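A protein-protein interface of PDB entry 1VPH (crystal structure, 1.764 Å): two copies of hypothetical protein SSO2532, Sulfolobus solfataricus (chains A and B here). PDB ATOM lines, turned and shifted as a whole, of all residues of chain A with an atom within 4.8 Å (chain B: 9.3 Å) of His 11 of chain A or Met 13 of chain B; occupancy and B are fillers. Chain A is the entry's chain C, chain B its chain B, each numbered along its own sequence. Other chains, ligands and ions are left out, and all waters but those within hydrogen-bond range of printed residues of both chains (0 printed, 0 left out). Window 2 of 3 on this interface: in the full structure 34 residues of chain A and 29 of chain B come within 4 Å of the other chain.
Met 13 of chain A touches its own counterpart, Met 13 of chain B.
Gly 148 of chain A touches Met 13 of chain B, but with the chains exchanged Met 13 of chain A does not touch Gly 148 of chain B (6.1 Å).
Of the 5 pairs that touch across the chains among the printed residues, 1 has its exchanged pair printed and touching as well.
ND1 of His 12 of chain A sits at hydrogen-bond distance from O of His 10 of chain A.
The side-chain sulfur of Met 13 of chain A lies within hydrogen-bond range of the backbone NH of Gly 148 of chain A (3.7 Å).
N of Ile 50 of chain B sits at hydrogen-bond distance from O of Leu 147 of chain B (2.8 Å).
ND1 of His 11 of chain A sits at hydrogen-bond distance from OE1 of Glu 149 of chain A (3.4 Å).
SD of Met 13 of chain B sits close to O of His 12 of chain A.
Of chain B, only Met 13 (3.7 Å) comes within 4 Å of His 11 of chain A.
Met 13 of chain B touches four residues of chain A.
Of chain B, only Met 13 (3.8 Å) comes within 4 Å of Gly 148 of chain A.
Of the printed residues of chain A, Leu 147 of chain B touches Met 13 (3.7 Å).
Printed residues of chain B within 4 Å of His 12 of chain A: Met 13 (3.6 Å).
Phe 17 of chain B touches none of the printed residues of chain A.
The nearest residue of chain B that does not touch His 11 of chain A is Lys 14 of chain B (5.8 Å).
The nearest printed residue of chain B that does not touch His 12 of chain A is Lys 14 of chain B (6.8 Å).
Among the printed residues, pairs that only touch across the chains: His 11 of chain A with Met 13 of chain B (3.7 Å), Met 13 of chain A with Met 13 of chain B (3.2 Å), Met 13 of chain A with Leu 147 of chain B (3.7 Å) and Gly 148 of chain A with Met 13 of chain B (3.8 Å).
Of the 7 printed residues of chain A, 4 touch a printed residue of chain B.
Printed residues of chain A that touch a printed residue of chain B: His 11, His 12, Met 13 and Gly 148.
Hydrophobic or aromatic side chains of chain A within 4 Å of the printed part of chain B: His 11 and Met 13.
Among the printed residues, no Asp or Glu carboxylate lies within 4 Å of a Lys or Arg side-chain nitrogen of the other chain.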
ATOM      1  N   HIS A   9      20.049  -1.061  41.312  1.00  0.00           N
ATOM      2  CA  HIS A   9      21.202  -0.209  41.057  1.00  0.00           C
ATOM      3  C   HIS A   9      21.949  -0.481  39.747  1.00  0.00           C
ATOM      4  O   HIS A   9      22.896   0.240  39.422  1.00  0.00           O
ATOM      5  CB  HIS A   9      22.103  -0.276  42.278  1.00  0.00           C
ATOM      6  CG  HIS A   9      21.483   0.373  43.476  1.00  0.00           C
ATOM      7  ND1 HIS A   9      20.579  -0.279  44.292  1.00  0.00           N
ATOM      8  CD2 HIS A   9      21.559   1.643  43.942  1.00  0.00           C
ATOM      9  CE1 HIS A   9      20.151   0.552  45.224  1.00  0.00           C
ATOM     10  NE2 HIS A   9      20.738   1.722  45.042  1.00  0.00           N
ATOM     11  N   HIS A  10      21.481  -1.455  38.957  1.00  0.00           N
ATOM     12  CA  HIS A  10      22.107  -1.801  37.718  1.00  0.00           C
ATOM     13  C   HIS A  10      20.996  -1.823  36.732  1.00  0.00           C
ATOM     14  O   HIS A  10      19.814  -1.992  37.131  1.00  0.00           O
ATOM     15  CB  HIS A  10      22.744  -3.181  37.811  1.00  0.00           C
ATOM     16  CG  HIS A  10      23.799  -3.268  38.868  1.00  0.00           C
ATOM     17  ND1 HIS A  10      23.524  -3.633  40.170  1.00  0.00           N
ATOM     18  CD2 HIS A  10      25.126  -2.993  38.820  1.00  0.00           C
ATOM     19  CE1 HIS A  10      24.643  -3.598  40.878  1.00  0.00           C
ATOM     20  NE2 HIS A  10      25.626  -3.205  40.085  1.00  0.00           N
ATOM     21  N   HIS A  11      21.389  -1.642  35.473  1.00  0.00           N
ATOM     22  CA  HIS A  11      20.491  -1.741  34.341  1.00  0.00           C
ATOM     23  C   HIS A  11      19.885  -3.143  34.422  1.00  0.00           C
ATOM     24  O   HIS A  11      20.524  -4.108  34.876  1.00  0.00           O
ATOM     25  CB  HIS A  11      21.234  -1.483  33.033  1.00  0.00           C
ATOM     26  CG  HIS A  11      21.634  -0.047  32.832  1.00  0.00           C
ATOM     27  ND1 HIS A  11      20.807   0.884  32.229  1.00  0.00           N
ATOM     28  CD2 HIS A  11      22.768   0.619  33.162  1.00  0.00           C
ATOM     29  CE1 HIS A  11      21.424   2.053  32.185  1.00  0.00           C
ATOM     30  NE2 HIS A  11      22.615   1.917  32.743  1.00  0.00           N
ATOM     31  N   HIS A  12      18.607  -3.222  34.121  1.00  0.00           N
ATOM     32  CA  HIS A  12      17.906  -4.490  34.254  1.00  0.00           C
ATOM     33  C   HIS A  12      16.759  -4.520  33.247  1.00  0.00           C
ATOM     34  O   HIS A  12      16.288  -3.477  32.779  1.00  0.00           O
ATOM     35  CB  HIS A  12      17.446  -4.691  35.693  1.00  0.00           C
ATOM     36  CG  HIS A  12      16.505  -3.635  36.173  1.00  0.00           C
ATOM     37  ND1 HIS A  12      16.948  -2.403  36.591  1.00  0.00           N
ATOM     38  CD2 HIS A  12      15.150  -3.601  36.259  1.00  0.00           C
ATOM     39  CE1 HIS A  12      15.910  -1.666  36.946  1.00  0.00           C
ATOM     40  NE2 HIS A  12      14.807  -2.367  36.759  1.00  0.00           N
ATOM     41  N   MET A  13      16.333  -5.735  32.920  1.00  0.00           N
ATOM     42  CA  MET A  13      15.302  -5.988  31.932  1.00  0.00           C
ATOM     43  C   MET A  13      13.922  -5.722  32.558  1.00  0.00           C
ATOM     44  O   MET A  13      13.679  -6.247  33.630  1.00  0.00           O
ATOM     45  CB  MET A  13      15.508  -7.478  31.479  1.00  0.00           C
ATOM     46  CG  MET A  13      14.408  -8.181  30.689  1.00  0.00           C
ATOM     47  SD  MET A  13      13.867  -7.171  29.310  1.00  0.00           S
ATOM     48  CE  MET A  13      15.297  -6.818  28.297  1.00  0.00           C
ATOM     49  N   GLY A 148      12.525  -4.112  27.752  1.00  0.00           N
ATOM     50  CA  GLY A 148      13.636  -3.174  27.647  1.00  0.00           C
ATOM     51  C   GLY A 148      13.956  -2.480  28.953  1.00  0.00           C
ATOM     52  O   GLY A 148      13.694  -3.037  30.016  1.00  0.00           O
ATOM     53  N   GLU A 149      14.511  -1.272  28.858  1.00  0.00           N
ATOM     54  CA  GLU A 149      14.921  -0.433  30.033  1.00  0.00           C
ATOM     55  C   GLU A 149      14.098   0.868  29.980  1.00  0.00           C
ATOM     56  O   GLU A 149      13.922   1.462  28.905  1.00  0.00           O
ATOM     57  CB  GLU A 149      16.461  -0.098  29.975  1.00  0.00           C
ATOM     58  CG  GLU A 149      16.847   0.974  28.868  1.00  0.00           C
ATOM     59  CD  GLU A 149      18.374   1.212  28.606  1.00  0.00           C
ATOM     60  OE1 GLU A 149      19.195   0.559  29.307  1.00  0.00           O
ATOM     61  OE2 GLU A 149      18.726   2.076  27.703  1.00  0.00           O
ATOM     62  OXT GLU A 149      13.601   1.420  30.977  1.00  0.00           O
ATOM     63  N   MET B  13      21.727  -5.876  31.564  1.00  0.00           N
ATOM     64  CA  MET B  13      21.042  -5.748  30.272  1.00  0.00           C
ATOM     65  C   MET B  13      21.656  -4.594  29.505  1.00  0.00           C
ATOM     66  O   MET B  13      22.149  -3.614  30.097  1.00  0.00           O
ATOM     67  CB  MET B  13      19.496  -5.634  30.441  1.00  0.00           C
ATOM     68  CG  MET B  13      18.827  -4.258  30.235  1.00  0.00           C
ATOM     69  SD  MET B  13      17.196  -4.426  29.386  1.00  0.00           S
ATOM     70  CE  MET B  13      17.744  -4.895  27.749  1.00  0.00           C
ATOM     71  N   LYS B  14      21.643  -4.705  28.180  1.00  0.00           N
ATOM     72  CA  LYS B  14      22.101  -3.614  27.344  1.00  0.00           C
ATOM     73  C   LYS B  14      21.211  -3.526  26.110  1.00  0.00           C
ATOM     74  O   LYS B  14      20.746  -4.533  25.660  1.00  0.00           O
ATOM     75  CB  LYS B  14      23.561  -3.874  26.915  1.00  0.00           C
ATOM     76  CG  LYS B  14      24.503  -4.424  28.047  1.00  0.00           C
ATOM     77  CD  LYS B  14      25.851  -4.973  27.527  1.00  0.00           C
ATOM     78  N   VAL B  15      20.945  -2.311  25.642  1.00  0.00           N
ATOM     79  CA  VAL B  15      20.161  -2.038  24.440  1.00  0.00           C
ATOM     80  C   VAL B  15      21.019  -1.066  23.617  1.00  0.00           C
ATOM     81  O   VAL B  15      21.470  -0.022  24.126  1.00  0.00           O
ATOM     82  CB  VAL B  15      18.828  -1.336  24.762  1.00  0.00           C
ATOM     83  CG1 VAL B  15      17.951  -1.241  23.529  1.00  0.00           C
ATOM     84  CG2 VAL B  15      18.096  -2.067  25.850  1.00  0.00           C
ATOM     85  N   TYR B  16      21.236  -1.389  22.363  1.00  0.00           N
ATOM     86  CA  TYR B  16      22.066  -0.602  21.519  1.00  0.00           C
ATOM     87  C   TYR B  16      21.352  -0.361  20.216  1.00  0.00           C
ATOM     88  O   TYR B  16      20.772  -1.278  19.679  1.00  0.00           O
ATOM     89  CB  TYR B  16      23.379  -1.347  21.292  1.00  0.00           C
ATOM     90  CG  TYR B  16      24.359  -0.618  20.449  1.00  0.00           C
ATOM     91  CD1 TYR B  16      25.190   0.356  20.984  1.00  0.00           C
ATOM     92  CD2 TYR B  16      24.495  -0.920  19.113  1.00  0.00           C
ATOM     93  CE1 TYR B  16      26.125   1.050  20.179  1.00  0.00           C
ATOM     94  CE2 TYR B  16      25.425  -0.257  18.312  1.00  0.00           C
ATOM     95  CZ  TYR B  16      26.238   0.728  18.830  1.00  0.00           C
ATOM     96  OH  TYR B  16      27.149   1.392  17.972  1.00  0.00           O
ATOM     97  N   PHE B  17      21.357   0.877  19.759  1.00  0.00           N
ATOM     98  CA  PHE B  17      20.720   1.225  18.489  1.00  0.00           C
ATOM     99  C   PHE B  17      21.747   1.774  17.505  1.00  0.00           C
ATOM    100  O   PHE B  17      22.667   2.531  17.883  1.00  0.00           O
ATOM    101  CB  PHE B  17      19.677   2.317  18.698  1.00  0.00           C
ATOM    102  CG  PHE B  17      18.517   1.910  19.512  1.00  0.00           C
ATOM    103  CD1 PHE B  17      17.393   1.386  18.924  1.00  0.00           C
ATOM    104  CD2 PHE B  17      18.514   2.132  20.870  1.00  0.00           C
ATOM    105  CE1 PHE B  17      16.279   1.026  19.712  1.00  0.00           C
ATOM    106  CE2 PHE B  17      17.429   1.774  21.639  1.00  0.00           C
ATOM    107  CZ  PHE B  17      16.322   1.222  21.068  1.00  0.00           C
ATOM    108  N   SER B  44      27.991  -3.080  19.324  1.00  0.00           N
ATOM    109  CA  SER B  44      27.155  -3.094  20.520  1.00  0.00           C
ATOM    110  C   SER B  44      27.857  -3.694  21.739  1.00  0.00           C
ATOM    111  O   SER B  44      27.503  -3.397  22.877  1.00  0.00           O
ATOM    112  CB  SER B  44      25.887  -3.919  20.302  1.00  0.00           C
ATOM    113  OG  SER B  44      26.186  -5.297  20.191  1.00  0.00           O
ATOM    114  N   ILE B  46      27.378  -6.599  22.703  1.00  0.00           N
ATOM    115  CA  ILE B  46      26.447  -7.552  23.304  1.00  0.00           C
ATOM    116  C   ILE B  46      26.832  -8.934  22.825  1.00  0.00           C
ATOM    117  O   ILE B  46      27.177  -9.120  21.664  1.00  0.00           O
ATOM    118  CB  ILE B  46      24.985  -7.194  22.976  1.00  0.00           C
ATOM    119  CG1 ILE B  46      24.606  -5.949  23.789  1.00  0.00           C
ATOM    120  CG2 ILE B  46      24.050  -8.326  23.286  1.00  0.00           C
ATOM    121  CD1 ILE B  46      23.541  -5.100  23.198  1.00  0.00           C
ATOM    122  N   ASN B  48      25.016 -12.019  23.957  1.00  0.00           N
ATOM    123  CA  ASN B  48      23.863 -12.893  23.880  1.00  0.00           C
ATOM    124  C   ASN B  48      22.578 -12.083  23.943  1.00  0.00           C
ATOM    125  O   ASN B  48      22.319 -11.353  24.911  1.00  0.00           O
ATOM    126  CB  ASN B  48      23.862 -13.934  24.994  1.00  0.00           C
ATOM    127  CG  ASN B  48      25.030 -14.911  24.906  1.00  0.00           C
ATOM    128  OD1 ASN B  48      25.147 -15.688  23.967  1.00  0.00           O
ATOM    129  ND2 ASN B  48      25.907 -14.872  25.913  1.00  0.00           N
ATOM    130  N   GLY B  49      21.766 -12.206  22.915  1.00  0.00           N
ATOM    131  CA  GLY B  49      20.561 -11.405  22.834  1.00  0.00           C
ATOM    132  C   GLY B  49      19.894 -11.555  21.475  1.00  0.00           C
ATOM    133  O   GLY B  49      19.910 -12.603  20.869  1.00  0.00           O
ATOM    134  N   ILE B  50      19.281 -10.470  21.023  1.00  0.00           N
ATOM    135  CA  ILE B  50      18.610 -10.468  19.751  1.00  0.00           C
ATOM    136  C   ILE B  50      19.044  -9.248  18.965  1.00  0.00           C
ATOM    137  O   ILE B  50      19.435  -8.240  19.542  1.00  0.00           O
ATOM    138  CB  ILE B  50      17.096 -10.487  19.867  1.00  0.00           C
ATOM    139  CG1 ILE B  50      16.574  -9.337  20.743  1.00  0.00           C
ATOM    140  CG2 ILE B  50      16.640 -11.861  20.452  1.00  0.00           C
ATOM    141  CD1 ILE B  50      15.102  -9.101  20.654  1.00  0.00           C
ATOM    142  N   GLU B 145      18.505  -2.637  16.241  1.00  0.00           N
ATOM    143  CA  GLU B 145      18.573  -2.673  17.671  1.00  0.00           C
ATOM    144  C   GLU B 145      19.135  -4.009  18.129  1.00  0.00           C
ATOM    145  O   GLU B 145      18.640  -5.096  17.761  1.00  0.00           O
ATOM    146  CB  GLU B 145      17.220  -2.422  18.359  1.00  0.00           C
ATOM    147  CG  GLU B 145      17.251  -2.495  19.870  1.00  0.00           C
ATOM    148  CD  GLU B 145      15.851  -2.343  20.494  1.00  0.00           C
ATOM    149  OE1 GLU B 145      14.918  -1.965  19.752  1.00  0.00           O
ATOM    150  OE2 GLU B 145      15.700  -2.669  21.691  1.00  0.00           O
ATOM    151  N   ILE B 146      20.134  -3.931  18.987  1.00  0.00           N
ATOM    152  CA  ILE B 146      20.664  -5.107  19.643  1.00  0.00           C
ATOM    153  C   ILE B 146      20.327  -5.030  21.149  1.00  0.00           C
ATOM    154  O   ILE B 146      20.545  -4.008  21.810  1.00  0.00           O
ATOM    155  CB  ILE B 146      22.149  -5.313  19.365  1.00  0.00           C
ATOM    156  CG1 ILE B 146      22.369  -5.525  17.867  1.00  0.00           C
ATOM    157  CG2 ILE B 146      22.633  -6.555  20.097  1.00  0.00           C
ATOM    158  CD1 ILE B 146      23.392  -4.644  17.309  1.00  0.00           C
ATOM    159  N   LEU B 147      19.718  -6.084  21.655  1.00  0.00           N
ATOM    160  CA  LEU B 147      19.209  -6.145  23.004  1.00  0.00           C
ATOM    161  C   LEU B 147      19.701  -7.443  23.622  1.00  0.00           C
ATOM    162  O   LEU B 147      19.555  -8.511  23.055  1.00  0.00           O
ATOM    163  CB  LEU B 147      17.672  -6.081  22.979  1.00  0.00           C
ATOM    164  CG  LEU B 147      16.898  -6.053  24.303  1.00  0.00           C
ATOM    165  CD1 LEU B 147      15.391  -6.017  23.994  1.00  0.00           C
ATOM    166  CD2 LEU B 147      17.215  -7.244  25.185  1.00  0.00           C
ATOM    167  N   GLY B 148      20.301  -7.367  24.793  1.00  0.00           N
ATOM    168  CA  GLY B 148      20.851  -8.574  25.358  1.00  0.00           C
ATOM    169  C   GLY B 148      21.820  -8.248  26.476  1.00  0.00           C
ATOM    170  O   GLY B 148      21.802  -7.149  27.030  1.00  0.00           O
ATOM    171  N   GLU B 149      22.678  -9.222  26.747  1.00  0.00           N
ATOM    172  CA  GLU B 149      23.744  -9.139  27.730  1.00  0.00           C
ATOM    173  C   GLU B 149      25.074  -9.378  27.039  1.00  0.00           C
ATOM    174  O   GLU B 149      25.160 -10.097  26.072  1.00  0.00           O
ATOM    175  CB  GLU B 149      23.554 -10.237  28.786  1.00  0.00           C
ATOM    176  CG  GLU B 149      23.985 -11.631  28.307  1.00  0.00           C
ATOM    177  CD  GLU B 149      23.567 -12.770  29.235  1.00  0.00           C
ATOM    178  OE1 GLU B 149      22.860 -12.507  30.240  1.00  0.00           O
ATOM    179  OE2 GLU B 149      23.945 -13.936  28.936  1.00  0.00           O
ATOM    180  OXT GLU B 149      26.116  -8.908  27.477  1.00  0.00           O
